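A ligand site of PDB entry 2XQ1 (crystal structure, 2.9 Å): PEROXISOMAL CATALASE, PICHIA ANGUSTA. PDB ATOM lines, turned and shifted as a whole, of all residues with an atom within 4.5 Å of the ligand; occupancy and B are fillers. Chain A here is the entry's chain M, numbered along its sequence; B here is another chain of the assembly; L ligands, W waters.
An oxygen (O2) of the ligand lies close to a ring nitrogen (NE2) of His 354 (3.3 Å).
The guanidinium group of Arg 64 is in salt-bridge range of an oxygen (O4) of the ligand (3.3 Å).
NH2 of Arg 357 is in salt-bridge range of O2 of the ligand (2.9 Å).
OH of Tyr 350 binds FE1 of the ligand, at 2.1 Å.
The guanidinium group of Arg 104 is in salt-bridge range of an oxygen (O3) of the ligand (2.9 Å).
OG1 of Thr 353 is in hydrogen-bond range of O of Asp 57 of chain B.
The backbone carbonyl oxygen (O) of Ser 106 sits at hydrogen-bond distance from the backbone NH (N) of Gly 123, 2.7 Å away.
O of Leu 291 sits at hydrogen-bond distance from N of Phe 145 (3.2 Å).
N of Phe 124 lies within hydrogen-bond range of O of Tyr 139 (2.7 Å).
O of Ala 125 sits at hydrogen-bond distance from N of Arg 104, 2.7 Å away.
The side-chain hydroxyl (OG) of Ser 349 lies within hydrogen-bond range of the side-chain carboxylate (OD1) of Asp 57 of chain B.
ND1 of His 354 sits close to O of Tyr 350 (3.3 Å).
A ring nitrogen (ND1) of His 67 is in hydrogen-bond range of the side-chain hydroxyl (OG) of Ser 106 (3.3 Å).
NE of Arg 346 sits close to N3 of the ligand (3.4 Å).
Merely in contact with the ligand: Val 65 (3.7 Å), Val 66 (3.4 Å), His 67 (3.2 Å), Ser 106 (3.8 Å), Gly 123 (3.3 Å), Phe 124 (3.6 Å), Val 138 (3.2 Å), Tyr 139 (3.5 Å), Asn 140 (2.9 Å), Pro 150 (3.8 Å), Phe 153 (3.3 Å), Ser 208 (3.8 Å), His 210 (3.5 Å), Leu 291 (3.7 Å), Phe 326 (3.0 Å), Val 342 (3.7 Å), Ser 345 (3.2 Å), Ser 349 (3.5 Å), Thr 353 (3.3 Å), Leu 53 of chain B (3.9 Å) and Asp 57 of chain B (3.8 Å).
27 residues have an atom within 4 Å of the ligand: Arg 64, Val 65, Val 66, His 67, Arg 104, Ser 106, Gly 123, Phe 124, Val 138, Tyr 139, Asn 140, Pro 150, Phe 153, Ser 208, His 210, Leu 291, Phe 326, Val 342, Ser 345, Arg 346, Ser 349, Tyr 350, Thr 353, His 354, Arg 357, Leu 53 of chain B and Asp 57 of chain B.
The nearest printed residue that does not touch the ligand is Ala 125 (4.04 Å).
Water W1 lies within hydrogen-bond range of N of Val 65 (2.7 Å), O1 of the ligand (2.8 Å) and OG1 of Thr 353 (3.0 Å).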
ATOM      1  N   ARG A  64       2.002  16.796 -14.866  1.00  0.00           N
ATOM      2  CA  ARG A  64       0.627  16.306 -14.883  1.00  0.00           C
ATOM      3  C   ARG A  64       0.396  15.415 -13.669  1.00  0.00           C
ATOM      4  O   ARG A  64       1.331  14.701 -13.284  1.00  0.00           O
ATOM      5  CB  ARG A  64       0.402  15.538 -16.169  1.00  0.00           C
ATOM      6  CG  ARG A  64       0.620  16.357 -17.477  1.00  0.00           C
ATOM      7  CD  ARG A  64       0.986  15.414 -18.642  1.00  0.00           C
ATOM      8  NE  ARG A  64       0.683  15.961 -19.956  1.00  0.00           N
ATOM      9  CZ  ARG A  64       1.497  16.788 -20.609  1.00  0.00           C
ATOM     10  NH1 ARG A  64       2.660  17.151 -20.053  1.00  0.00           N
ATOM     11  NH2 ARG A  64       1.176  17.239 -21.811  1.00  0.00           N
ATOM     12  N   VAL A  65      -0.785  15.454 -13.022  1.00  0.00           N
ATOM     13  CA  VAL A  65      -0.984  14.603 -11.823  1.00  0.00           C
ATOM     14  C   VAL A  65      -0.655  13.137 -12.131  1.00  0.00           C
ATOM     15  O   VAL A  65      -0.101  12.410 -11.250  1.00  0.00           O
ATOM     16  CB  VAL A  65      -2.408  14.608 -11.269  1.00  0.00           C
ATOM     17  CG1 VAL A  65      -2.759  15.918 -10.722  1.00  0.00           C
ATOM     18  CG2 VAL A  65      -3.419  14.217 -12.350  1.00  0.00           C
ATOM     19  N   VAL A  66      -1.045  12.723 -13.354  1.00  0.00           N
ATOM     20  CA  VAL A  66      -0.773  11.395 -13.897  1.00  0.00           C
ATOM     21  C   VAL A  66      -0.229  11.531 -15.332  1.00  0.00           C
ATOM     22  O   VAL A  66      -0.393  12.563 -15.969  1.00  0.00           O
ATOM     23  CB  VAL A  66      -2.041  10.515 -13.917  1.00  0.00           C
ATOM     24  CG1 VAL A  66      -2.499  10.191 -12.491  1.00  0.00           C
ATOM     25  CG2 VAL A  66      -3.138  11.198 -14.703  1.00  0.00           C
ATOM     26  N   HIS A  67       0.422  10.477 -15.827  1.00  0.00           N
ATOM     27  CA  HIS A  67       1.018  10.479 -17.175  1.00  0.00           C
ATOM     28  C   HIS A  67       2.083  11.576 -17.309  1.00  0.00           C
ATOM     29  O   HIS A  67       2.247  12.202 -18.371  1.00  0.00           O
ATOM     30  CB  HIS A  67      -0.070  10.610 -18.266  1.00  0.00           C
ATOM     31  CG  HIS A  67      -1.043   9.467 -18.299  1.00  0.00           C
ATOM     32  ND1 HIS A  67      -0.933   8.424 -19.206  1.00  0.00           N
ATOM     33  CD2 HIS A  67      -2.133   9.192 -17.550  1.00  0.00           C
ATOM     34  CE1 HIS A  67      -1.924   7.570 -19.007  1.00  0.00           C
ATOM     35  NE2 HIS A  67      -2.664   8.003 -18.017  1.00  0.00           N
ATOM     36  N   ARG A 104       0.955  12.225 -28.015  1.00  0.00           N
ATOM     37  CA  ARG A 104       1.833  12.143 -26.853  1.00  0.00           C
ATOM     38  C   ARG A 104       1.716  10.782 -26.189  1.00  0.00           C
ATOM     39  O   ARG A 104       0.611  10.346 -25.848  1.00  0.00           O
ATOM     40  CB  ARG A 104       1.534  13.283 -25.846  1.00  0.00           C
ATOM     41  CG  ARG A 104       2.511  13.301 -24.655  1.00  0.00           C
ATOM     42  CD  ARG A 104       2.044  14.216 -23.556  1.00  0.00           C
ATOM     43  NE  ARG A 104       3.172  14.517 -22.670  1.00  0.00           N
ATOM     44  CZ  ARG A 104       3.325  14.023 -21.434  1.00  0.00           C
ATOM     45  NH1 ARG A 104       2.411  13.220 -20.891  1.00  0.00           N
ATOM     46  NH2 ARG A 104       4.404  14.371 -20.734  1.00  0.00           N
ATOM     47  N   SER A 106       3.089   8.197 -23.011  1.00  0.00           N
ATOM     48  CA  SER A 106       3.315   8.424 -21.596  1.00  0.00           C
ATOM     49  C   SER A 106       3.153   7.124 -20.843  1.00  0.00           C
ATOM     50  O   SER A 106       2.457   6.212 -21.310  1.00  0.00           O
ATOM     51  CB  SER A 106       2.245   9.380 -21.069  1.00  0.00           C
ATOM     52  OG  SER A 106       0.990   9.209 -21.765  1.00  0.00           O
ATOM     53  N   GLY A 123      -0.053   5.678 -22.165  1.00  0.00           N
ATOM     54  CA  GLY A 123      -1.016   6.667 -22.645  1.00  0.00           C
ATOM     55  C   GLY A 123      -0.736   6.940 -24.093  1.00  0.00           C
ATOM     56  O   GLY A 123       0.422   6.939 -24.499  1.00  0.00           O
ATOM     57  N   PHE A 124      -1.777   7.165 -24.867  1.00  0.00           N
ATOM     58  CA  PHE A 124      -1.663   7.315 -26.312  1.00  0.00           C
ATOM     59  C   PHE A 124      -2.661   8.384 -26.675  1.00  0.00           C
ATOM     60  O   PHE A 124      -3.803   8.079 -27.025  1.00  0.00           O
ATOM     61  CB  PHE A 124      -2.083   5.978 -26.965  1.00  0.00           C
ATOM     62  CG  PHE A 124      -1.712   5.815 -28.433  1.00  0.00           C
ATOM     63  CD1 PHE A 124      -1.937   6.830 -29.368  1.00  0.00           C
ATOM     64  CD2 PHE A 124      -1.161   4.603 -28.896  1.00  0.00           C
ATOM     65  CE1 PHE A 124      -1.600   6.657 -30.723  1.00  0.00           C
ATOM     66  CE2 PHE A 124      -0.830   4.409 -30.249  1.00  0.00           C
ATOM     67  CZ  PHE A 124      -1.046   5.446 -31.164  1.00  0.00           C
ATOM     68  N   ALA A 125      -2.253   9.648 -26.568  1.00  0.00           N
ATOM     69  CA  ALA A 125      -3.185  10.773 -26.789  1.00  0.00           C
ATOM     70  C   ALA A 125      -2.901  11.531 -28.089  1.00  0.00           C
ATOM     71  O   ALA A 125      -1.737  11.906 -28.389  1.00  0.00           O
ATOM     72  CB  ALA A 125      -3.153  11.732 -25.603  1.00  0.00           C
ATOM     73  N   VAL A 138      -8.032  10.558 -26.439  1.00  0.00           N
ATOM     74  CA  VAL A 138      -7.154  10.380 -25.294  1.00  0.00           C
ATOM     75  C   VAL A 138      -7.245   8.928 -24.880  1.00  0.00           C
ATOM     76  O   VAL A 138      -8.088   8.568 -24.033  1.00  0.00           O
ATOM     77  CB  VAL A 138      -7.543  11.306 -24.093  1.00  0.00           C
ATOM     78  CG1 VAL A 138      -6.455  11.271 -22.986  1.00  0.00           C
ATOM     79  CG2 VAL A 138      -7.809  12.746 -24.548  1.00  0.00           C
ATOM     80  N   TYR A 139      -6.398   8.099 -25.489  1.00  0.00           N
ATOM     81  CA  TYR A 139      -6.528   6.639 -25.391  1.00  0.00           C
ATOM     82  C   TYR A 139      -5.416   5.996 -24.578  1.00  0.00           C
ATOM     83  O   TYR A 139      -4.333   6.556 -24.440  1.00  0.00           O
ATOM     84  CB  TYR A 139      -6.521   6.009 -26.780  1.00  0.00           C
ATOM     85  CG  TYR A 139      -7.700   6.311 -27.675  1.00  0.00           C
ATOM     86  CD1 TYR A 139      -8.741   7.129 -27.257  1.00  0.00           C
ATOM     87  CD2 TYR A 139      -7.784   5.757 -28.971  1.00  0.00           C
ATOM     88  CE1 TYR A 139      -9.813   7.410 -28.083  1.00  0.00           C
ATOM     89  CE2 TYR A 139      -8.871   6.030 -29.823  1.00  0.00           C
ATOM     90  CZ  TYR A 139      -9.872   6.860 -29.356  1.00  0.00           C
ATOM     91  OH  TYR A 139     -10.967   7.149 -30.126  1.00  0.00           O
ATOM     92  N   ASN A 140      -5.673   4.809 -24.050  1.00  0.00           N
ATOM     93  CA  ASN A 140      -4.614   3.984 -23.472  1.00  0.00           C
ATOM     94  C   ASN A 140      -4.189   2.838 -24.382  1.00  0.00           C
ATOM     95  O   ASN A 140      -4.790   2.633 -25.450  1.00  0.00           O
ATOM     96  CB  ASN A 140      -5.026   3.462 -22.102  1.00  0.00           C
ATOM     97  CG  ASN A 140      -4.755   4.473 -21.010  1.00  0.00           C
ATOM     98  OD1 ASN A 140      -3.810   5.251 -21.121  1.00  0.00           O
ATOM     99  ND2 ASN A 140      -5.583   4.479 -19.953  1.00  0.00           N
ATOM    100  N   PHE A 145      -9.698  -0.948 -18.258  1.00  0.00           N
ATOM    101  CA  PHE A 145      -9.066  -0.187 -17.185  1.00  0.00           C
ATOM    102  C   PHE A 145      -9.399  -0.725 -15.821  1.00  0.00           C
ATOM    103  O   PHE A 145     -10.232  -1.620 -15.691  1.00  0.00           O
ATOM    104  CB  PHE A 145      -9.410   1.307 -17.275  1.00  0.00           C
ATOM    105  CG  PHE A 145      -8.378   2.222 -16.643  1.00  0.00           C
ATOM    106  CD1 PHE A 145      -7.052   2.239 -17.104  1.00  0.00           C
ATOM    107  CD2 PHE A 145      -8.725   3.071 -15.601  1.00  0.00           C
ATOM    108  CE1 PHE A 145      -6.099   3.092 -16.529  1.00  0.00           C
ATOM    109  CE2 PHE A 145      -7.778   3.936 -15.021  1.00  0.00           C
ATOM    110  CZ  PHE A 145      -6.471   3.929 -15.492  1.00  0.00           C
ATOM    111  N   ILE A 147     -10.828   0.605 -13.311  1.00  0.00           N
ATOM    112  CA  ILE A 147     -12.027   1.097 -12.615  1.00  0.00           C
ATOM    113  C   ILE A 147     -13.209   1.364 -13.535  1.00  0.00           C
ATOM    114  O   ILE A 147     -13.050   1.502 -14.736  1.00  0.00           O
ATOM    115  CB  ILE A 147     -11.723   2.385 -11.821  1.00  0.00           C
ATOM    116  CG1 ILE A 147     -11.320   3.545 -12.756  1.00  0.00           C
ATOM    117  CG2 ILE A 147     -10.617   2.106 -10.800  1.00  0.00           C
ATOM    118  CD1 ILE A 147     -11.655   4.899 -12.192  1.00  0.00           C
ATOM    119  N   PRO A 150     -16.177   6.438 -11.433  1.00  0.00           N
ATOM    120  CA  PRO A 150     -15.296   7.570 -11.716  1.00  0.00           C
ATOM    121  C   PRO A 150     -14.590   8.044 -10.477  1.00  0.00           C
ATOM    122  O   PRO A 150     -13.380   8.159 -10.481  1.00  0.00           O
ATOM    123  CB  PRO A 150     -16.249   8.642 -12.239  1.00  0.00           C
ATOM    124  CG  PRO A 150     -17.592   8.230 -11.741  1.00  0.00           C
ATOM    125  CD  PRO A 150     -17.588   6.750 -11.714  1.00  0.00           C
ATOM    126  N   PHE A 153     -11.061   6.985  -8.992  1.00  0.00           N
ATOM    127  CA  PHE A 153      -9.788   7.266  -9.640  1.00  0.00           C
ATOM    128  C   PHE A 153      -8.715   7.794  -8.676  1.00  0.00           C
ATOM    129  O   PHE A 153      -7.601   7.237  -8.646  1.00  0.00           O
ATOM    130  CB  PHE A 153      -9.955   8.192 -10.835  1.00  0.00           C
ATOM    131  CG  PHE A 153      -8.778   8.232 -11.730  1.00  0.00           C
ATOM    132  CD1 PHE A 153      -8.469   7.151 -12.552  1.00  0.00           C
ATOM    133  CD2 PHE A 153      -7.966   9.349 -11.740  1.00  0.00           C
ATOM    134  CE1 PHE A 153      -7.362   7.181 -13.387  1.00  0.00           C
ATOM    135  CE2 PHE A 153      -6.870   9.407 -12.575  1.00  0.00           C
ATOM    136  CZ  PHE A 153      -6.556   8.313 -13.402  1.00  0.00           C
ATOM    137  N   SER A 208      -9.625   3.128 -27.625  1.00  0.00           N
ATOM    138  CA  SER A 208     -10.476   4.139 -27.009  1.00  0.00           C
ATOM    139  C   SER A 208     -10.827   3.743 -25.557  1.00  0.00           C
ATOM    140  O   SER A 208     -11.097   4.601 -24.694  1.00  0.00           O
ATOM    141  CB  SER A 208     -11.755   4.334 -27.830  1.00  0.00           C
ATOM    142  OG  SER A 208     -12.609   3.223 -27.656  1.00  0.00           O
ATOM    143  N   HIS A 210     -13.186   3.370 -23.711  1.00  0.00           N
ATOM    144  CA  HIS A 210     -14.605   3.647 -23.500  1.00  0.00           C
ATOM    145  C   HIS A 210     -15.315   3.410 -24.786  1.00  0.00           C
ATOM    146  O   HIS A 210     -14.698   3.272 -25.833  1.00  0.00           O
ATOM    147  CB  HIS A 210     -14.868   5.091 -23.115  1.00  0.00           C
ATOM    148  CG  HIS A 210     -14.085   5.563 -21.940  1.00  0.00           C
ATOM    149  ND1 HIS A 210     -14.374   5.183 -20.641  1.00  0.00           N
ATOM    150  CD2 HIS A 210     -13.023   6.405 -21.862  1.00  0.00           C
ATOM    151  CE1 HIS A 210     -13.514   5.757 -19.823  1.00  0.00           C
ATOM    152  NE2 HIS A 210     -12.679   6.510 -20.536  1.00  0.00           N
ATOM    153  N   LEU A 291     -16.056   0.047 -18.350  1.00  0.00           N
ATOM    154  CA  LEU A 291     -14.722   0.213 -18.881  1.00  0.00           C
ATOM    155  C   LEU A 291     -13.848  -1.008 -18.622  1.00  0.00           C
ATOM    156  O   LEU A 291     -12.738  -1.111 -19.155  1.00  0.00           O
ATOM    157  CB  LEU A 291     -14.115   1.514 -18.337  1.00  0.00           C
ATOM    158  CG  LEU A 291     -12.669   1.892 -18.675  1.00  0.00           C
ATOM    159  CD1 LEU A 291     -12.511   2.314 -20.130  1.00  0.00           C
ATOM    160  CD2 LEU A 291     -12.301   3.009 -17.766  1.00  0.00           C
ATOM    161  N   PHE A 326      -4.721  17.672 -23.679  1.00  0.00           N
ATOM    162  CA  PHE A 326      -5.803  16.932 -24.308  1.00  0.00           C
ATOM    163  C   PHE A 326      -6.972  16.794 -23.344  1.00  0.00           C
ATOM    164  O   PHE A 326      -6.752  16.722 -22.144  1.00  0.00           O
ATOM    165  CB  PHE A 326      -5.353  15.518 -24.626  1.00  0.00           C
ATOM    166  CG  PHE A 326      -4.111  15.429 -25.431  1.00  0.00           C
ATOM    167  CD1 PHE A 326      -4.153  15.501 -26.823  1.00  0.00           C
ATOM    168  CD2 PHE A 326      -2.879  15.191 -24.800  1.00  0.00           C
ATOM    169  CE1 PHE A 326      -2.972  15.374 -27.590  1.00  0.00           C
ATOM    170  CE2 PHE A 326      -1.692  15.071 -25.533  1.00  0.00           C
ATOM    171  CZ  PHE A 326      -1.736  15.171 -26.935  1.00  0.00           C
ATOM    172  N   VAL A 342     -16.966   6.674 -16.103  1.00  0.00           N
ATOM    173  CA  VAL A 342     -15.558   7.051 -16.034  1.00  0.00           C
ATOM    174  C   VAL A 342     -15.283   8.120 -17.080  1.00  0.00           C
ATOM    175  O   VAL A 342     -14.796   9.223 -16.756  1.00  0.00           O
ATOM    176  CB  VAL A 342     -14.618   5.862 -16.202  1.00  0.00           C
ATOM    177  CG1 VAL A 342     -13.157   6.321 -16.272  1.00  0.00           C
ATOM    178  CG2 VAL A 342     -14.804   4.933 -15.045  1.00  0.00           C
ATOM    179  N   SER A 345     -16.847  11.593 -16.219  1.00  0.00           N
ATOM    180  CA  SER A 345     -16.131  12.432 -15.276  1.00  0.00           C
ATOM    181  C   SER A 345     -14.873  12.998 -15.940  1.00  0.00           C
ATOM    182  O   SER A 345     -14.418  14.109 -15.635  1.00  0.00           O
ATOM    183  CB  SER A 345     -15.776  11.612 -14.037  1.00  0.00           C
ATOM    184  OG  SER A 345     -14.695  10.746 -14.345  1.00  0.00           O
ATOM    185  N   ARG A 346     -14.299  12.220 -16.854  1.00  0.00           N
ATOM    186  CA  ARG A 346     -13.103  12.671 -17.543  1.00  0.00           C
ATOM    187  C   ARG A 346     -13.412  13.948 -18.289  1.00  0.00           C
ATOM    188  O   ARG A 346     -12.523  14.789 -18.419  1.00  0.00           O
ATOM    189  CB  ARG A 346     -12.562  11.596 -18.479  1.00  0.00           C
ATOM    190  CG  ARG A 346     -11.821  10.496 -17.776  1.00  0.00           C
ATOM    191  CD  ARG A 346     -11.388   9.419 -18.724  1.00  0.00           C
ATOM    192  NE  ARG A 346     -10.177   9.715 -19.495  1.00  0.00           N
ATOM    193  CZ  ARG A 346      -9.985   9.283 -20.751  1.00  0.00           C
ATOM    194  NH1 ARG A 346     -10.927   8.580 -21.374  1.00  0.00           N
ATOM    195  NH2 ARG A 346      -8.854   9.584 -21.403  1.00  0.00           N
ATOM    196  N   SER A 349     -12.703  16.652 -15.629  1.00  0.00           N
ATOM    197  CA  SER A 349     -11.305  16.711 -15.126  1.00  0.00           C
ATOM    198  C   SER A 349     -10.247  17.392 -16.005  1.00  0.00           C
ATOM    199  O   SER A 349      -9.440  18.190 -15.529  1.00  0.00           O
ATOM    200  CB  SER A 349     -10.736  15.319 -14.928  1.00  0.00           C
ATOM    201  OG  SER A 349     -10.929  14.878 -13.621  1.00  0.00           O
ATOM    202  N   TYR A 350     -10.200  17.003 -17.267  1.00  0.00           N
ATOM    203  CA  TYR A 350      -9.036  17.322 -18.051  1.00  0.00           C
ATOM    204  C   TYR A 350      -8.965  18.846 -18.200  1.00  0.00           C
ATOM    205  O   TYR A 350      -7.985  19.437 -17.760  1.00  0.00           O
ATOM    206  CB  TYR A 350      -9.024  16.551 -19.378  1.00  0.00           C
ATOM    207  CG  TYR A 350      -8.693  15.048 -19.281  1.00  0.00           C
ATOM    208  CD1 TYR A 350      -9.552  14.153 -18.645  1.00  0.00           C
ATOM    209  CD2 TYR A 350      -7.537  14.512 -19.855  1.00  0.00           C
ATOM    210  CE1 TYR A 350      -9.264  12.758 -18.581  1.00  0.00           C
ATOM    211  CE2 TYR A 350      -7.254  13.136 -19.805  1.00  0.00           C
ATOM    212  CZ  TYR A 350      -8.116  12.265 -19.171  1.00  0.00           C
ATOM    213  OH  TYR A 350      -7.856  10.916 -19.110  1.00  0.00           O
ATOM    214  N   THR A 353      -7.984  20.380 -14.773  1.00  0.00           N
ATOM    215  CA  THR A 353      -6.586  20.281 -14.473  1.00  0.00           C
ATOM    216  C   THR A 353      -5.740  21.177 -15.409  1.00  0.00           C
ATOM    217  O   THR A 353      -4.738  21.774 -14.978  1.00  0.00           O
ATOM    218  CB  THR A 353      -6.130  18.812 -14.490  1.00  0.00           C
ATOM    219  OG1 THR A 353      -4.975  18.657 -13.655  1.00  0.00           O
ATOM    220  CG2 THR A 353      -5.769  18.363 -15.889  1.00  0.00           C
ATOM    221  N   HIS A 354      -6.121  21.301 -16.677  1.00  0.00           N
ATOM    222  CA  HIS A 354      -5.380  22.218 -17.574  1.00  0.00           C
ATOM    223  C   HIS A 354      -5.338  23.662 -17.013  1.00  0.00           C
ATOM    224  O   HIS A 354      -4.272  24.313 -17.000  1.00  0.00           O
ATOM    225  CB  HIS A 354      -6.010  22.302 -18.968  1.00  0.00           C
ATOM    226  CG  HIS A 354      -6.078  21.007 -19.708  1.00  0.00           C
ATOM    227  ND1 HIS A 354      -7.067  20.725 -20.627  1.00  0.00           N
ATOM    228  CD2 HIS A 354      -5.293  19.906 -19.639  1.00  0.00           C
ATOM    229  CE1 HIS A 354      -6.880  19.506 -21.108  1.00  0.00           C
ATOM    230  NE2 HIS A 354      -5.818  18.986 -20.526  1.00  0.00           N
ATOM    231  N   ARG A 357      -2.571  23.290 -14.244  1.00  0.00           N
ATOM    232  CA  ARG A 357      -1.220  22.993 -14.711  1.00  0.00           C
ATOM    233  C   ARG A 357      -0.651  24.100 -15.610  1.00  0.00           C
ATOM    234  O   ARG A 357       0.493  24.479 -15.446  1.00  0.00           O
ATOM    235  CB  ARG A 357      -1.188  21.641 -15.429  1.00  0.00           C
ATOM    236  CG  ARG A 357       0.182  21.230 -15.972  1.00  0.00           C
ATOM    237  CD  ARG A 357       0.204  19.769 -16.379  1.00  0.00           C
ATOM    238  NE  ARG A 357      -0.554  19.528 -17.613  1.00  0.00           N
ATOM    239  CZ  ARG A 357      -0.055  19.676 -18.838  1.00  0.00           C
ATOM    240  NH1 ARG A 357       1.237  20.045 -19.010  1.00  0.00           N
ATOM    241  NH2 ARG A 357      -0.840  19.457 -19.903  1.00  0.00           N
ATOM    242  N   LEU B  53     -12.713  15.462  -7.248  1.00  0.00           N
ATOM    243  CA  LEU B  53     -11.978  15.476  -8.524  1.00  0.00           C
ATOM    244  C   LEU B  53     -11.201  16.767  -8.681  1.00  0.00           C
ATOM    245  O   LEU B  53     -10.031  16.757  -9.048  1.00  0.00           O
ATOM    246  CB  LEU B  53     -12.888  15.247  -9.734  1.00  0.00           C
ATOM    247  CG  LEU B  53     -13.094  13.767 -10.054  1.00  0.00           C
ATOM    248  CD1 LEU B  53     -13.880  13.528 -11.352  1.00  0.00           C
ATOM    249  CD2 LEU B  53     -11.750  13.119 -10.154  1.00  0.00           C
ATOM    250  N   ASP B  57      -7.283  17.169  -9.271  1.00  0.00           N
ATOM    251  CA  ASP B  57      -6.754  17.906 -10.403  1.00  0.00           C
ATOM    252  C   ASP B  57      -5.684  18.910  -9.971  1.00  0.00           C
ATOM    253  O   ASP B  57      -4.857  19.348 -10.799  1.00  0.00           O
ATOM    254  CB  ASP B  57      -7.885  18.628 -11.142  1.00  0.00           C
ATOM    255  CG  ASP B  57      -8.899  17.674 -11.779  1.00  0.00           C
ATOM    256  OD1 ASP B  57      -8.559  16.488 -12.029  1.00  0.00           O
ATOM    257  OD2 ASP B  57     -10.047  18.116 -12.059  1.00  0.00           O
HETATM  258  C1  LIG L   1      -3.953  12.220 -18.213  1.00  0.00           C
HETATM  259  C2  LIG L   1      -7.704  12.409 -15.161  1.00  0.00           C
HETATM  260  C3  LIG L   1      -8.896   7.940 -16.633  1.00  0.00           C
HETATM  261  C4  LIG L   1      -5.931   8.285 -20.472  1.00  0.00           C
HETATM  262  C5  LIG L   1      -4.809  12.695 -17.250  1.00  0.00           C
HETATM  263  C6  LIG L   1      -4.745  13.952 -16.526  1.00  0.00           C
HETATM  264  C7  LIG L   1      -5.798  13.987 -15.675  1.00  0.00           C
HETATM  265  C8  LIG L   1      -6.559  12.764 -15.846  1.00  0.00           C
HETATM  266  C9  LIG L   1      -6.190  15.108 -14.677  1.00  0.00           C
HETATM  267  C10 LIG L   1      -3.641  15.054 -16.711  1.00  0.00           C
HETATM  268  C11 LIG L   1      -3.815  15.805 -18.029  1.00  0.00           C
HETATM  269  C12 LIG L   1      -3.194  17.180 -17.939  1.00  0.00           C
HETATM  270  O1  LIG L   1      -2.722  17.525 -16.818  1.00  0.00           O
HETATM  271  O2  LIG L   1      -3.172  17.941 -18.950  1.00  0.00           O
HETATM  272  C13 LIG L   1      -8.333  11.199 -15.228  1.00  0.00           C
HETATM  273  C14 LIG L   1      -9.426  10.729 -14.417  1.00  0.00           C
HETATM  274  C15 LIG L   1      -9.752   9.498 -14.822  1.00  0.00           C
HETATM  275  C16 LIG L   1      -8.886   9.132 -15.924  1.00  0.00           C
HETATM  276  C17 LIG L   1     -10.103  11.535 -13.278  1.00  0.00           C
HETATM  277  C18 LIG L   1     -10.851   8.574 -14.265  1.00  0.00           C
HETATM  278  C19 LIG L   1     -12.050   9.043 -13.965  1.00  0.00           C
HETATM  279  C20 LIG L   1      -8.330   7.680 -17.869  1.00  0.00           C
HETATM  280  C21 LIG L   1      -8.696   6.652 -18.829  1.00  0.00           C
HETATM  281  C22 LIG L   1      -7.868   6.749 -19.889  1.00  0.00           C
HETATM  282  C23 LIG L   1      -6.944   7.829 -19.654  1.00  0.00           C
HETATM  283  C24 LIG L   1      -9.838   5.624 -18.626  1.00  0.00           C
HETATM  284  C25 LIG L   1      -7.870   5.877 -21.148  1.00  0.00           C
HETATM  285  C26 LIG L   1      -8.777   6.181 -22.071  1.00  0.00           C
HETATM  286  C27 LIG L   1      -5.074   9.332 -20.177  1.00  0.00           C
HETATM  287  C28 LIG L   1      -3.888   9.669 -20.911  1.00  0.00           C
HETATM  288  C29 LIG L   1      -3.261  10.880 -20.219  1.00  0.00           C
HETATM  289  C30 LIG L   1      -4.146  11.182 -19.110  1.00  0.00           C
HETATM  290  C31 LIG L   1      -3.339   8.966 -22.161  1.00  0.00           C
HETATM  291  C32 LIG L   1      -2.001  11.609 -20.668  1.00  0.00           C
HETATM  292  C33 LIG L   1      -2.421  12.623 -21.735  1.00  0.00           C
HETATM  293  C34 LIG L   1      -1.211  13.414 -22.149  1.00  0.00           C
HETATM  294  O3  LIG L   1      -0.093  12.833 -22.376  1.00  0.00           O
HETATM  295  O4  LIG L   1      -1.371  14.655 -22.230  1.00  0.00           O
HETATM  296  N1  LIG L   1      -5.927  12.015 -16.801  1.00  0.00           N
HETATM  297  N2  LIG L   1      -8.039  10.199 -16.126  1.00  0.00           N
HETATM  298  N3  LIG L   1      -7.274   8.368 -18.423  1.00  0.00           N
HETATM  299  N4  LIG L   1      -5.181  10.238 -19.131  1.00  0.00           N
HETATM  300 FE1  LIG L   1      -6.607  10.202 -17.646  1.00  0.00          FE
HETATM  301  O   HOH W   1      -2.296  17.416 -14.092  1.00  0.00           O
